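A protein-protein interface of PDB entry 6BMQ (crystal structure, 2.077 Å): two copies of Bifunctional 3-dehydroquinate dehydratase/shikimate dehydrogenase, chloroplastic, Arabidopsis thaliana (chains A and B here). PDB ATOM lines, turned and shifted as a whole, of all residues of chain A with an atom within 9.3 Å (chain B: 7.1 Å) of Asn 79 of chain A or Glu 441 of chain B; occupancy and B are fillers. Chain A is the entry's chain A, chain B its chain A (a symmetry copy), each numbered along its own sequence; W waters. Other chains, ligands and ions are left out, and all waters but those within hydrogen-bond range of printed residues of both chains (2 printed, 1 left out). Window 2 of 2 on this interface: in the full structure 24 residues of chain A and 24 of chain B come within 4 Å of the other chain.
No position is printed for both chains.
Of the printed residues of chain B, Trp 69 of chain A touches Pro 438.
Of the printed residues of chain B, Asp 77 of chain A touches Asn 519 (3.7 Å).
Asn 79 of chain A touches two residues of chain B.
Arg 81 of chain A touches none of the printed residues of chain B.
Of the printed residues of chain B, Gln 101 of chain A touches Pro 438 and Asn 439.
Printed residues of chain B within 4 Å of Glu 105 of chain A: Asn 439 (2.7 Å), Val 440 (3.7 Å), Glu 441 (3.3 Å) and Glu 442 (3.6 Å).
Of chain A, only Glu 78 (3.96 Å), Asn 79 (3.7 Å) and Glu 105 (3.7 Å) come within 4 Å of Val 440 of chain B.
Glu 441 of chain B touches three residues of chain A.
Of the printed residues of chain A, Asn 519 of chain B touches Gly 76 (3.3 Å) and Asp 77 (3.7 Å).
The nearest residue of chain B that does not touch Asn 79 of chain A is Arg 470 of chain B (5.5 Å).
Among the printed residues, merely in contact across the chains: Trp 69 of chain A with Pro 438 of chain B, Gly 76 of chain A with Asn 519 of chain B, Asp 77 of chain A with Asn 519 of chain B, Glu 78 of chain A with Pro 438 of chain B, Glu 78 of chain A with Val 440 of chain B, Asn 79 of chain A with Val 440 of chain B, Arg 82 of chain A with Glu 441 of chain B, Gln 101 of chain A with Pro 438 of chain B, Val 102 of chain A with Pro 438 of chain B, Val 102 of chain A with Asn 439 of chain B, Glu 105 of chain A with Val 440 of chain B and Glu 105 of chain A with Glu 442 of chain B.
The side-chain carboxylate of Asp 77 of chain A is in hydrogen-bond range of the backbone NH of Asn 79 of chain A, 3.1 Å away.
OE2 of Glu 78 of chain A is in salt-bridge range of NE of Arg 82 of chain A, 2.9 Å away.
The guanidinium group of Arg 82 of chain A is in salt-bridge range of the side-chain carboxylate of Glu 105 of chain A (2.9 Å).
The backbone NH of Gly 435 of chain B lies within hydrogen-bond range of the side-chain carboxylate of Glu 442 of chain B, 3.1 Å away.
NE of Arg 467 of chain B lies within salt-bridge range of OE2 of Glu 441 of chain B (3.9 Å).
OE2 of Glu 441 of chain B is in salt-bridge range of NH2 of Arg 470 of chain B (3.5 Å).
Water W2 bridges the side-chain amino group of Lys 108 of chain A (2.7 Å) and the backbone carbonyl oxygen of Glu 441 of chain B (3.3 Å).
Water W1 lies within hydrogen-bond range of ND2 of Asn 519 of chain B (2.7 Å) and OD1 of Asp 77 of chain A (2.8 Å).
Hydrophobic or aromatic side chains of chain A within 4 Å of the printed part of chain B: Trp 69 and Val 102.
Among the printed residues, 17 pairs touch across the chains.
The side-chain carboxylate (OE1) of Glu 441 of chain B lies within hydrogen-bond range of the side-chain amide nitrogen (ND2) of Asn 79 of chain A (3.5 Å).
The backbone carbonyl oxygen (O) of Pro 438 of chain B lies within hydrogen-bond range of the guanidinium group (NH2) of Arg 82 of chain A (2.8 Å).
The side-chain amide nitrogen (NE2) of Gln 101 of chain A sits close to the side-chain amide nitrogen (ND2) of Asn 439 of chain B.
OE2 of Glu 105 of chain A sits close to OD1 of Asn 439 of chain B (2.7 Å).
OE1 of Glu 105 of chain A is in hydrogen-bond range of N of Glu 441 of chain B.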
ATOM      1  N   TYR A  65      12.656  -5.398  39.152  1.00  0.00           N
ATOM      2  CA  TYR A  65      13.659  -4.836  38.250  1.00  0.00           C
ATOM      3  C   TYR A  65      12.915  -4.462  36.980  1.00  0.00           C
ATOM      4  O   TYR A  65      12.961  -5.177  35.983  1.00  0.00           O
ATOM      5  CB  TYR A  65      14.786  -5.846  38.019  1.00  0.00           C
ATOM      6  CG  TYR A  65      16.140  -5.296  37.625  1.00  0.00           C
ATOM      7  CD1 TYR A  65      16.443  -3.934  37.739  1.00  0.00           C
ATOM      8  CD2 TYR A  65      17.154  -6.162  37.224  1.00  0.00           C
ATOM      9  CE1 TYR A  65      17.704  -3.451  37.420  1.00  0.00           C
ATOM     10  CE2 TYR A  65      18.423  -5.680  36.894  1.00  0.00           C
ATOM     11  CZ  TYR A  65      18.692  -4.326  36.991  1.00  0.00           C
ATOM     12  OH  TYR A  65      19.948  -3.841  36.668  1.00  0.00           O
ATOM     13  N   TRP A  69       9.687  -1.310  29.007  1.00  0.00           N
ATOM     14  CA  TRP A  69       8.449  -1.723  28.338  1.00  0.00           C
ATOM     15  C   TRP A  69       7.308  -2.056  29.312  1.00  0.00           C
ATOM     16  O   TRP A  69       6.217  -2.438  28.892  1.00  0.00           O
ATOM     17  CB  TRP A  69       8.700  -2.911  27.392  1.00  0.00           C
ATOM     18  CG  TRP A  69       9.575  -4.037  27.922  1.00  0.00           C
ATOM     19  CD1 TRP A  69      10.915  -4.199  27.712  1.00  0.00           C
ATOM     20  CD2 TRP A  69       9.154  -5.166  28.708  1.00  0.00           C
ATOM     21  NE1 TRP A  69      11.361  -5.343  28.334  1.00  0.00           N
ATOM     22  CE2 TRP A  69      10.302  -5.954  28.954  1.00  0.00           C
ATOM     23  CE3 TRP A  69       7.926  -5.576  29.245  1.00  0.00           C
ATOM     24  CZ2 TRP A  69      10.255  -7.122  29.707  1.00  0.00           C
ATOM     25  CZ3 TRP A  69       7.879  -6.736  29.995  1.00  0.00           C
ATOM     26  CH2 TRP A  69       9.035  -7.498  30.217  1.00  0.00           C
ATOM     27  N   TYR A  74      14.607   0.285  33.704  1.00  0.00           N
ATOM     28  CA  TYR A  74      15.691  -0.567  33.230  1.00  0.00           C
ATOM     29  C   TYR A  74      15.723  -0.685  31.717  1.00  0.00           C
ATOM     30  O   TYR A  74      14.720  -1.036  31.085  1.00  0.00           O
ATOM     31  CB  TYR A  74      15.604  -1.980  33.823  1.00  0.00           C
ATOM     32  CG  TYR A  74      16.655  -2.921  33.254  1.00  0.00           C
ATOM     33  CD1 TYR A  74      17.956  -2.929  33.756  1.00  0.00           C
ATOM     34  CD2 TYR A  74      16.350  -3.794  32.206  1.00  0.00           C
ATOM     35  CE1 TYR A  74      18.920  -3.790  33.246  1.00  0.00           C
ATOM     36  CE2 TYR A  74      17.316  -4.661  31.686  1.00  0.00           C
ATOM     37  CZ  TYR A  74      18.595  -4.648  32.214  1.00  0.00           C
ATOM     38  OH  TYR A  74      19.559  -5.485  31.710  1.00  0.00           O
ATOM     39  N   GLY A  76      18.431  -2.464  28.674  1.00  0.00           N
ATOM     40  CA  GLY A  76      19.561  -3.360  28.539  1.00  0.00           C
ATOM     41  C   GLY A  76      19.143  -4.792  28.325  1.00  0.00           C
ATOM     42  O   GLY A  76      18.006  -5.075  27.941  1.00  0.00           O
ATOM     43  N   ASP A  77      20.082  -5.699  28.571  1.00  0.00           N
ATOM     44  CA  ASP A  77      19.898  -7.112  28.272  1.00  0.00           C
ATOM     45  C   ASP A  77      18.851  -7.752  29.174  1.00  0.00           C
ATOM     46  O   ASP A  77      18.859  -7.555  30.394  1.00  0.00           O
ATOM     47  CB  ASP A  77      21.230  -7.850  28.405  1.00  0.00           C
ATOM     48  CG  ASP A  77      21.151  -9.270  27.921  1.00  0.00           C
ATOM     49  OD1 ASP A  77      21.261  -9.484  26.698  1.00  0.00           O
ATOM     50  OD2 ASP A  77      20.977 -10.175  28.762  1.00  0.00           O
ATOM     51  N   GLU A  78      17.961  -8.524  28.560  1.00  0.00           N
ATOM     52  CA  GLU A  78      16.817  -9.102  29.256  1.00  0.00           C
ATOM     53  C   GLU A  78      17.212 -10.276  30.148  1.00  0.00           C
ATOM     54  O   GLU A  78      16.687 -10.426  31.258  1.00  0.00           O
ATOM     55  CB  GLU A  78      15.749  -9.533  28.245  1.00  0.00           C
ATOM     56  CG  GLU A  78      14.603 -10.323  28.837  1.00  0.00           C
ATOM     57  CD  GLU A  78      13.813  -9.559  29.882  1.00  0.00           C
ATOM     58  OE1 GLU A  78      13.967  -8.324  29.996  1.00  0.00           O
ATOM     59  OE2 GLU A  78      13.021 -10.206  30.591  1.00  0.00           O
ATOM     60  N   ASN A  79      18.145 -11.096  29.670  1.00  0.00           N
ATOM     61  CA  ASN A  79      18.671 -12.203  30.462  1.00  0.00           C
ATOM     62  C   ASN A  79      19.407 -11.708  31.699  1.00  0.00           C
ATOM     63  O   ASN A  79      19.299 -12.303  32.763  1.00  0.00           O
ATOM     64  CB  ASN A  79      19.596 -13.081  29.604  1.00  0.00           C
ATOM     65  CG  ASN A  79      18.826 -14.081  28.773  1.00  0.00           C
ATOM     66  OD1 ASN A  79      17.976 -14.810  29.292  1.00  0.00           O
ATOM     67  ND2 ASN A  79      19.082 -14.094  27.469  1.00  0.00           N
ATOM     68  N   GLU A  80      20.150 -10.612  31.569  1.00  0.00           N
ATOM     69  CA  GLU A  80      20.830 -10.056  32.732  1.00  0.00           C
ATOM     70  C   GLU A  80      19.811  -9.580  33.770  1.00  0.00           C
ATOM     71  O   GLU A  80      20.002  -9.757  34.971  1.00  0.00           O
ATOM     72  CB  GLU A  80      21.767  -8.919  32.319  1.00  0.00           C
ATOM     73  CG  GLU A  80      22.983  -9.428  31.542  1.00  0.00           C
ATOM     74  CD  GLU A  80      23.839  -8.322  30.947  1.00  0.00           C
ATOM     75  OE1 GLU A  80      24.689  -8.639  30.084  1.00  0.00           O
ATOM     76  OE2 GLU A  80      23.671  -7.147  31.337  1.00  0.00           O
ATOM     77  N   ARG A  81      18.709  -9.005  33.301  1.00  0.00           N
ATOM     78  CA  ARG A  81      17.652  -8.558  34.202  1.00  0.00           C
ATOM     79  C   ARG A  81      17.047  -9.729  34.981  1.00  0.00           C
ATOM     80  O   ARG A  81      16.841  -9.643  36.189  1.00  0.00           O
ATOM     81  CB  ARG A  81      16.568  -7.836  33.418  1.00  0.00           C
ATOM     82  CG  ARG A  81      15.610  -7.022  34.257  1.00  0.00           C
ATOM     83  CD  ARG A  81      14.524  -6.419  33.360  1.00  0.00           C
ATOM     84  NE  ARG A  81      13.650  -7.432  32.781  1.00  0.00           N
ATOM     85  CZ  ARG A  81      12.582  -7.953  33.394  1.00  0.00           C
ATOM     86  NH1 ARG A  81      12.250  -7.586  34.636  1.00  0.00           N
ATOM     87  NH2 ARG A  81      11.849  -8.858  32.761  1.00  0.00           N
ATOM     88  N   ARG A  82      16.767 -10.821  34.282  1.00  0.00           N
ATOM     89  CA  ARG A  82      16.242 -12.013  34.924  1.00  0.00           C
ATOM     90  C   ARG A  82      17.259 -12.639  35.880  1.00  0.00           C
ATOM     91  O   ARG A  82      16.869 -13.152  36.928  1.00  0.00           O
ATOM     92  CB  ARG A  82      15.807 -13.038  33.881  1.00  0.00           C
ATOM     93  CG  ARG A  82      14.767 -12.513  32.904  1.00  0.00           C
ATOM     94  CD  ARG A  82      14.389 -13.583  31.893  1.00  0.00           C
ATOM     95  NE  ARG A  82      13.547 -13.049  30.825  1.00  0.00           N
ATOM     96  CZ  ARG A  82      12.978 -13.792  29.873  1.00  0.00           C
ATOM     97  NH1 ARG A  82      13.155 -15.109  29.851  1.00  0.00           N
ATOM     98  NH2 ARG A  82      12.234 -13.209  28.940  1.00  0.00           N
ATOM     99  N   ASP A  83      18.544 -12.597  35.520  1.00  0.00           N
ATOM    100  CA  ASP A  83      19.615 -13.124  36.385  1.00  0.00           C
ATOM    101  C   ASP A  83      19.593 -12.474  37.760  1.00  0.00           C
ATOM    102  O   ASP A  83      19.744 -13.144  38.772  1.00  0.00           O
ATOM    103  CB  ASP A  83      20.995 -12.898  35.760  1.00  0.00           C
ATOM    104  CG  ASP A  83      21.327 -13.913  34.676  1.00  0.00           C
ATOM    105  OD1 ASP A  83      20.656 -14.973  34.623  1.00  0.00           O
ATOM    106  OD2 ASP A  83      22.270 -13.652  33.894  1.00  0.00           O
ATOM    107  N   VAL A  84      19.414 -11.156  37.774  1.00  0.00           N
ATOM    108  CA  VAL A  84      19.294 -10.381  39.007  1.00  0.00           C
ATOM    109  C   VAL A  84      18.115 -10.854  39.863  1.00  0.00           C
ATOM    110  O   VAL A  84      18.257 -11.075  41.066  1.00  0.00           O
ATOM    111  CB  VAL A  84      19.142  -8.891  38.681  1.00  0.00           C
ATOM    112  CG1 VAL A  84      18.703  -8.109  39.891  1.00  0.00           C
ATOM    113  CG2 VAL A  84      20.468  -8.343  38.108  1.00  0.00           C
ATOM    114  N   LEU A  85      16.955 -11.025  39.240  1.00  0.00           N
ATOM    115  CA  LEU A  85      15.778 -11.487  39.972  1.00  0.00           C
ATOM    116  C   LEU A  85      15.996 -12.900  40.523  1.00  0.00           C
ATOM    117  O   LEU A  85      15.656 -13.174  41.676  1.00  0.00           O
ATOM    118  CB  LEU A  85      14.523 -11.437  39.085  1.00  0.00           C
ATOM    119  CG  LEU A  85      14.046 -10.048  38.616  1.00  0.00           C
ATOM    120  CD1 LEU A  85      12.757 -10.134  37.791  1.00  0.00           C
ATOM    121  CD2 LEU A  85      13.828  -9.147  39.791  1.00  0.00           C
ATOM    122  N   ARG A  86      16.576 -13.785  39.717  1.00  0.00           N
ATOM    123  CA  ARG A  86      16.880 -15.135  40.184  1.00  0.00           C
ATOM    124  C   ARG A  86      17.863 -15.065  41.347  1.00  0.00           C
ATOM    125  O   ARG A  86      17.749 -15.803  42.324  1.00  0.00           O
ATOM    126  CB  ARG A  86      17.437 -16.003  39.046  1.00  0.00           C
ATOM    127  CG  ARG A  86      16.358 -16.606  38.147  1.00  0.00           C
ATOM    128  CD  ARG A  86      16.914 -17.563  37.089  1.00  0.00           C
ATOM    129  NE  ARG A  86      17.728 -16.867  36.091  1.00  0.00           N
ATOM    130  CZ  ARG A  86      17.285 -16.486  34.896  1.00  0.00           C
ATOM    131  NH1 ARG A  86      16.030 -16.723  34.535  1.00  0.00           N
ATOM    132  NH2 ARG A  86      18.100 -15.852  34.064  1.00  0.00           N
ATOM    133  N   LEU A  87      18.816 -14.149  41.247  1.00  0.00           N
ATOM    134  CA  LEU A  87      19.809 -13.978  42.288  1.00  0.00           C
ATOM    135  C   LEU A  87      19.144 -13.505  43.580  1.00  0.00           C
ATOM    136  O   LEU A  87      19.410 -14.047  44.655  1.00  0.00           O
ATOM    137  CB  LEU A  87      20.890 -12.995  41.832  1.00  0.00           C
ATOM    138  CG  LEU A  87      22.153 -12.836  42.677  1.00  0.00           C
ATOM    139  CD1 LEU A  87      22.855 -14.182  42.844  1.00  0.00           C
ATOM    140  CD2 LEU A  87      23.099 -11.820  42.039  1.00  0.00           C
ATOM    141  N   GLN A 101       4.446 -10.667  30.758  1.00  0.00           N
ATOM    142  CA  GLN A 101       4.998 -10.899  29.420  1.00  0.00           C
ATOM    143  C   GLN A 101       6.093 -11.978  29.370  1.00  0.00           C
ATOM    144  O   GLN A 101       6.162 -12.715  28.396  1.00  0.00           O
ATOM    145  CB  GLN A 101       5.549  -9.577  28.861  1.00  0.00           C
ATOM    146  CG  GLN A 101       6.221  -9.651  27.489  1.00  0.00           C
ATOM    147  CD  GLN A 101       5.247  -9.920  26.342  1.00  0.00           C
ATOM    148  OE1 GLN A 101       4.023  -9.904  26.517  1.00  0.00           O
ATOM    149  NE2 GLN A 101       5.798 -10.159  25.155  1.00  0.00           N
ATOM    150  N   VAL A 102       6.951 -12.052  30.391  1.00  0.00           N
ATOM    151  CA  VAL A 102       8.033 -13.045  30.420  1.00  0.00           C
ATOM    152  C   VAL A 102       7.908 -14.073  31.568  1.00  0.00           C
ATOM    153  O   VAL A 102       8.845 -14.851  31.827  1.00  0.00           O
ATOM    154  CB  VAL A 102       9.418 -12.354  30.529  1.00  0.00           C
ATOM    155  CG1 VAL A 102       9.636 -11.380  29.341  1.00  0.00           C
ATOM    156  CG2 VAL A 102       9.552 -11.631  31.862  1.00  0.00           C
ATOM    157  N   SER A 104       6.154 -16.883  32.104  1.00  0.00           N
ATOM    158  CA  SER A 104       6.201 -18.329  31.829  1.00  0.00           C
ATOM    159  C   SER A 104       7.626 -18.825  31.745  1.00  0.00           C
ATOM    160  O   SER A 104       7.999 -19.780  32.429  1.00  0.00           O
ATOM    161  CB  SER A 104       5.476 -18.676  30.534  1.00  0.00           C
ATOM    162  OG  SER A 104       4.077 -18.564  30.702  1.00  0.00           O
ATOM    163  N   GLU A 105       8.407 -18.169  30.890  1.00  0.00           N
ATOM    164  CA  GLU A 105       9.831 -18.452  30.737  1.00  0.00           C
ATOM    165  C   GLU A 105      10.521 -18.389  32.080  1.00  0.00           C
ATOM    166  O   GLU A 105      11.286 -19.280  32.447  1.00  0.00           O
ATOM    167  CB  GLU A 105      10.503 -17.447  29.789  1.00  0.00           C
ATOM    168  CG  GLU A 105      10.181 -17.588  28.318  1.00  0.00           C
ATOM    169  CD  GLU A 105      10.343 -16.268  27.565  1.00  0.00           C
ATOM    170  OE1 GLU A 105      11.439 -15.662  27.592  1.00  0.00           O
ATOM    171  OE2 GLU A 105       9.346 -15.830  26.960  1.00  0.00           O
ATOM    172  N   PHE A 106      10.258 -17.311  32.813  1.00  0.00           N
ATOM    173  CA  PHE A 106      10.999 -17.072  34.034  1.00  0.00           C
ATOM    174  C   PHE A 106      10.718 -18.135  35.097  1.00  0.00           C
ATOM    175  O   PHE A 106      11.635 -18.632  35.743  1.00  0.00           O
ATOM    176  CB  PHE A 106      10.684 -15.702  34.603  1.00  0.00           C
ATOM    177  CG  PHE A 106      11.462 -15.400  35.828  1.00  0.00           C
ATOM    178  CD1 PHE A 106      12.747 -14.904  35.729  1.00  0.00           C
ATOM    179  CD2 PHE A 106      10.933 -15.658  37.082  1.00  0.00           C
ATOM    180  CE1 PHE A 106      13.489 -14.629  36.873  1.00  0.00           C
ATOM    181  CE2 PHE A 106      11.668 -15.394  38.229  1.00  0.00           C
ATOM    182  CZ  PHE A 106      12.951 -14.878  38.122  1.00  0.00           C
ATOM    183  N   LYS A 108       9.524 -21.135  34.647  1.00  0.00           N
ATOM    184  CA  LYS A 108      10.189 -22.344  34.169  1.00  0.00           C
ATOM    185  C   LYS A 108      11.668 -22.378  34.572  1.00  0.00           C
ATOM    186  O   LYS A 108      12.193 -23.437  34.905  1.00  0.00           O
ATOM    187  CB  LYS A 108      10.056 -22.477  32.644  1.00  0.00           C
ATOM    188  CG  LYS A 108       8.677 -22.971  32.200  1.00  0.00           C
ATOM    189  CD  LYS A 108       8.638 -23.338  30.710  1.00  0.00           C
ATOM    190  CE  LYS A 108       8.830 -22.126  29.829  1.00  0.00           C
ATOM    191  NZ  LYS A 108       9.210 -22.490  28.416  1.00  0.00           N
ATOM    192  N   SER A 109      12.335 -21.230  34.561  1.00  0.00           N
ATOM    193  CA  SER A 109      13.766 -21.197  34.874  1.00  0.00           C
ATOM    194  C   SER A 109      14.098 -21.505  36.336  1.00  0.00           C
ATOM    195  O   SER A 109      15.240 -21.852  36.656  1.00  0.00           O
ATOM    196  CB  SER A 109      14.356 -19.834  34.534  1.00  0.00           C
ATOM    197  OG  SER A 109      13.982 -18.894  35.523  1.00  0.00           O
ATOM    198  N   GLY B 435      10.147 -15.857  20.483  1.00  0.00           N
ATOM    199  CA  GLY B 435      11.546 -15.495  20.538  1.00  0.00           C
ATOM    200  C   GLY B 435      11.819 -13.995  20.459  1.00  0.00           C
ATOM    201  O   GLY B 435      12.931 -13.565  20.744  1.00  0.00           O
ATOM    202  N   MET B 436      10.818 -13.205  20.066  1.00  0.00           N
ATOM    203  CA  MET B 436      10.988 -11.754  19.945  1.00  0.00           C
ATOM    204  C   MET B 436      11.123 -11.101  21.310  1.00  0.00           C
ATOM    205  O   MET B 436      10.454 -11.523  22.252  1.00  0.00           O
ATOM    206  CB  MET B 436       9.814 -11.133  19.189  1.00  0.00           C
ATOM    207  CG  MET B 436       9.990  -9.642  18.843  1.00  0.00           C
ATOM    208  SD  MET B 436       8.667  -8.974  17.779  1.00  0.00           S
ATOM    209  CE  MET B 436       7.431  -8.567  19.018  1.00  0.00           C
ATOM    210  N   PRO B 438      10.608  -8.933  24.490  1.00  0.00           N
ATOM    211  CA  PRO B 438      11.538  -9.420  25.515  1.00  0.00           C
ATOM    212  C   PRO B 438      11.483 -10.923  25.788  1.00  0.00           C
ATOM    213  O   PRO B 438      11.978 -11.351  26.833  1.00  0.00           O
ATOM    214  CB  PRO B 438      11.077  -8.664  26.761  1.00  0.00           C
ATOM    215  CG  PRO B 438       9.584  -8.648  26.596  1.00  0.00           C
ATOM    216  CD  PRO B 438       9.346  -8.456  25.095  1.00  0.00           C
ATOM    217  N   ASN B 439      10.892 -11.705  24.893  1.00  0.00           N
ATOM    218  CA  ASN B 439      10.788 -13.150  25.119  1.00  0.00           C
ATOM    219  C   ASN B 439      11.953 -13.924  24.531  1.00  0.00           C
ATOM    220  O   ASN B 439      11.788 -14.799  23.673  1.00  0.00           O
ATOM    221  CB  ASN B 439       9.476 -13.677  24.561  1.00  0.00           C
ATOM    222  CG  ASN B 439       8.276 -13.124  25.309  1.00  0.00           C
ATOM    223  OD1 ASN B 439       8.011 -13.491  26.463  1.00  0.00           O
ATOM    224  ND2 ASN B 439       7.552 -12.232  24.663  1.00  0.00           N
ATOM    225  N   VAL B 440      13.134 -13.605  25.030  1.00  0.00           N
ATOM    226  CA  VAL B 440      14.366 -14.043  24.409  1.00  0.00           C
ATOM    227  C   VAL B 440      14.702 -15.511  24.679  1.00  0.00           C
ATOM    228  O   VAL B 440      15.539 -16.085  23.981  1.00  0.00           O
ATOM    229  CB  VAL B 440      15.516 -13.163  24.881  1.00  0.00           C
ATOM    230  CG1 VAL B 440      15.257 -11.705  24.462  1.00  0.00           C
ATOM    231  CG2 VAL B 440      15.639 -13.256  26.386  1.00  0.00           C
ATOM    232  N   GLU B 441      14.060 -16.123  25.678  1.00  0.00           N
ATOM    233  CA  GLU B 441      14.303 -17.547  25.971  1.00  0.00           C
ATOM    234  C   GLU B 441      13.183 -18.443  25.491  1.00  0.00           C
ATOM    235  O   GLU B 441      13.182 -19.639  25.770  1.00  0.00           O
ATOM    236  CB  GLU B 441      14.509 -17.777  27.461  1.00  0.00           C
ATOM    237  CG  GLU B 441      15.863 -17.352  27.934  1.00  0.00           C
ATOM    238  CD  GLU B 441      16.973 -17.978  27.109  1.00  0.00           C
ATOM    239  OE1 GLU B 441      17.896 -17.245  26.696  1.00  0.00           O
ATOM    240  OE2 GLU B 441      16.929 -19.207  26.886  1.00  0.00           O
ATOM    241  N   GLU B 442      12.219 -17.851  24.792  1.00  0.00           N
ATOM    242  CA  GLU B 442      11.163 -18.604  24.135  1.00  0.00           C
ATOM    243  C   GLU B 442      11.629 -19.086  22.767  1.00  0.00           C
ATOM    244  O   GLU B 442      12.076 -18.287  21.947  1.00  0.00           O
ATOM    245  CB  GLU B 442       9.911 -17.742  23.982  1.00  0.00           C
ATOM    246  CG  GLU B 442       8.751 -18.435  23.294  1.00  0.00           C
ATOM    247  CD  GLU B 442       7.631 -17.468  22.938  1.00  0.00           C
ATOM    248  OE1 GLU B 442       7.928 -16.308  22.561  1.00  0.00           O
ATOM    249  OE2 GLU B 442       6.450 -17.871  23.040  1.00  0.00           O
ATOM    250  N   THR B 443      11.544 -20.392  22.527  1.00  0.00           N
ATOM    251  CA  THR B 443      11.808 -20.937  21.198  1.00  0.00           C
ATOM    252  C   THR B 443      10.617 -21.792  20.766  1.00  0.00           C
ATOM    253  O   THR B 443       9.952 -22.400  21.598  1.00  0.00           O
ATOM    254  CB  THR B 443      13.108 -21.760  21.156  1.00  0.00           C
ATOM    255  OG1 THR B 443      13.273 -22.321  19.848  1.00  0.00           O
ATOM    256  CG2 THR B 443      13.096 -22.887  22.204  1.00  0.00           C
ATOM    257  N   THR B 466      18.072 -15.066  18.024  1.00  0.00           N
ATOM    258  CA  THR B 466      17.033 -15.613  18.889  1.00  0.00           C
ATOM    259  C   THR B 466      17.537 -16.874  19.571  1.00  0.00           C
ATOM    260  O   THR B 466      18.629 -17.355  19.254  1.00  0.00           O
ATOM    261  CB  THR B 466      15.744 -15.939  18.111  1.00  0.00           C
ATOM    262  OG1 THR B 466      16.053 -16.717  16.943  1.00  0.00           O
ATOM    263  CG2 THR B 466      15.051 -14.662  17.680  1.00  0.00           C
ATOM    264  N   ARG B 467      16.764 -17.411  20.509  1.00  0.00           N
ATOM    265  CA  ARG B 467      17.104 -18.715  21.072  1.00  0.00           C
ATOM    266  C   ARG B 467      17.086 -19.766  19.958  1.00  0.00           C
ATOM    267  O   ARG B 467      17.939 -20.651  19.913  1.00  0.00           O
ATOM    268  CB  ARG B 467      16.145 -19.120  22.199  1.00  0.00           C
ATOM    269  CG  ARG B 467      16.563 -20.418  22.897  1.00  0.00           C
ATOM    270  CD  ARG B 467      15.556 -20.891  23.940  1.00  0.00           C
ATOM    271  NE  ARG B 467      15.937 -22.184  24.511  1.00  0.00           N
ATOM    272  CZ  ARG B 467      15.235 -22.837  25.431  1.00  0.00           C
ATOM    273  NH1 ARG B 467      14.098 -22.327  25.888  1.00  0.00           N
ATOM    274  NH2 ARG B 467      15.662 -24.010  25.880  1.00  0.00           N
ATOM    275  N   ARG B 470      20.221 -19.440  17.821  1.00  0.00           N
ATOM    276  CA  ARG B 470      21.383 -19.796  18.629  1.00  0.00           C
ATOM    277  C   ARG B 470      21.536 -21.307  18.684  1.00  0.00           C
ATOM    278  O   ARG B 470      22.588 -21.848  18.359  1.00  0.00           O
ATOM    279  CB  ARG B 470      21.263 -19.229  20.045  1.00  0.00           C
ATOM    280  CG  ARG B 470      22.445 -19.562  20.949  1.00  0.00           C
ATOM    281  CD  ARG B 470      22.321 -18.917  22.324  1.00  0.00           C
ATOM    282  NE  ARG B 470      21.276 -19.540  23.134  1.00  0.00           N
ATOM    283  CZ  ARG B 470      20.227 -18.892  23.633  1.00  0.00           C
ATOM    284  NH1 ARG B 470      20.082 -17.589  23.407  1.00  0.00           N
ATOM    285  NH2 ARG B 470      19.323 -19.541  24.363  1.00  0.00           N
ATOM    286  N   GLU B 471      20.467 -21.981  19.090  1.00  0.00           N
ATOM    287  CA  GLU B 471      20.487 -23.423  19.275  1.00  0.00           C
ATOM    288  C   GLU B 471      20.618 -24.158  17.952  1.00  0.00           C
ATOM    289  O   GLU B 471      21.172 -25.252  17.889  1.00  0.00           O
ATOM    290  CB  GLU B 471      19.225 -23.869  20.014  1.00  0.00           C
ATOM    291  CG  GLU B 471      19.212 -23.391  21.444  1.00  0.00           C
ATOM    292  CD  GLU B 471      17.993 -23.831  22.189  1.00  0.00           C
ATOM    293  OE1 GLU B 471      17.047 -24.311  21.534  1.00  0.00           O
ATOM    294  OE2 GLU B 471      17.989 -23.698  23.432  1.00  0.00           O
ATOM    295  N   ASN B 519      17.847  -4.703  22.132  1.00  0.00           N
ATOM    296  CA  ASN B 519      16.987  -4.319  23.249  1.00  0.00           C
ATOM    297  C   ASN B 519      16.496  -2.890  23.160  1.00  0.00           C
ATOM    298  O   ASN B 519      16.404  -2.209  24.173  1.00  0.00           O
ATOM    299  CB  ASN B 519      17.710  -4.518  24.577  1.00  0.00           C
ATOM    300  CG  ASN B 519      18.198  -5.928  24.748  1.00  0.00           C
ATOM    301  OD1 ASN B 519      17.403  -6.865  24.912  1.00  0.00           O
ATOM    302  ND2 ASN B 519      19.507  -6.099  24.704  1.00  0.00           N
HETATM  303  O   HOH W   1      20.350  -8.656  24.166  1.00  0.00           O
HETATM  304  O   HOH W   2      11.310 -20.880  28.236  1.00  0.00           O
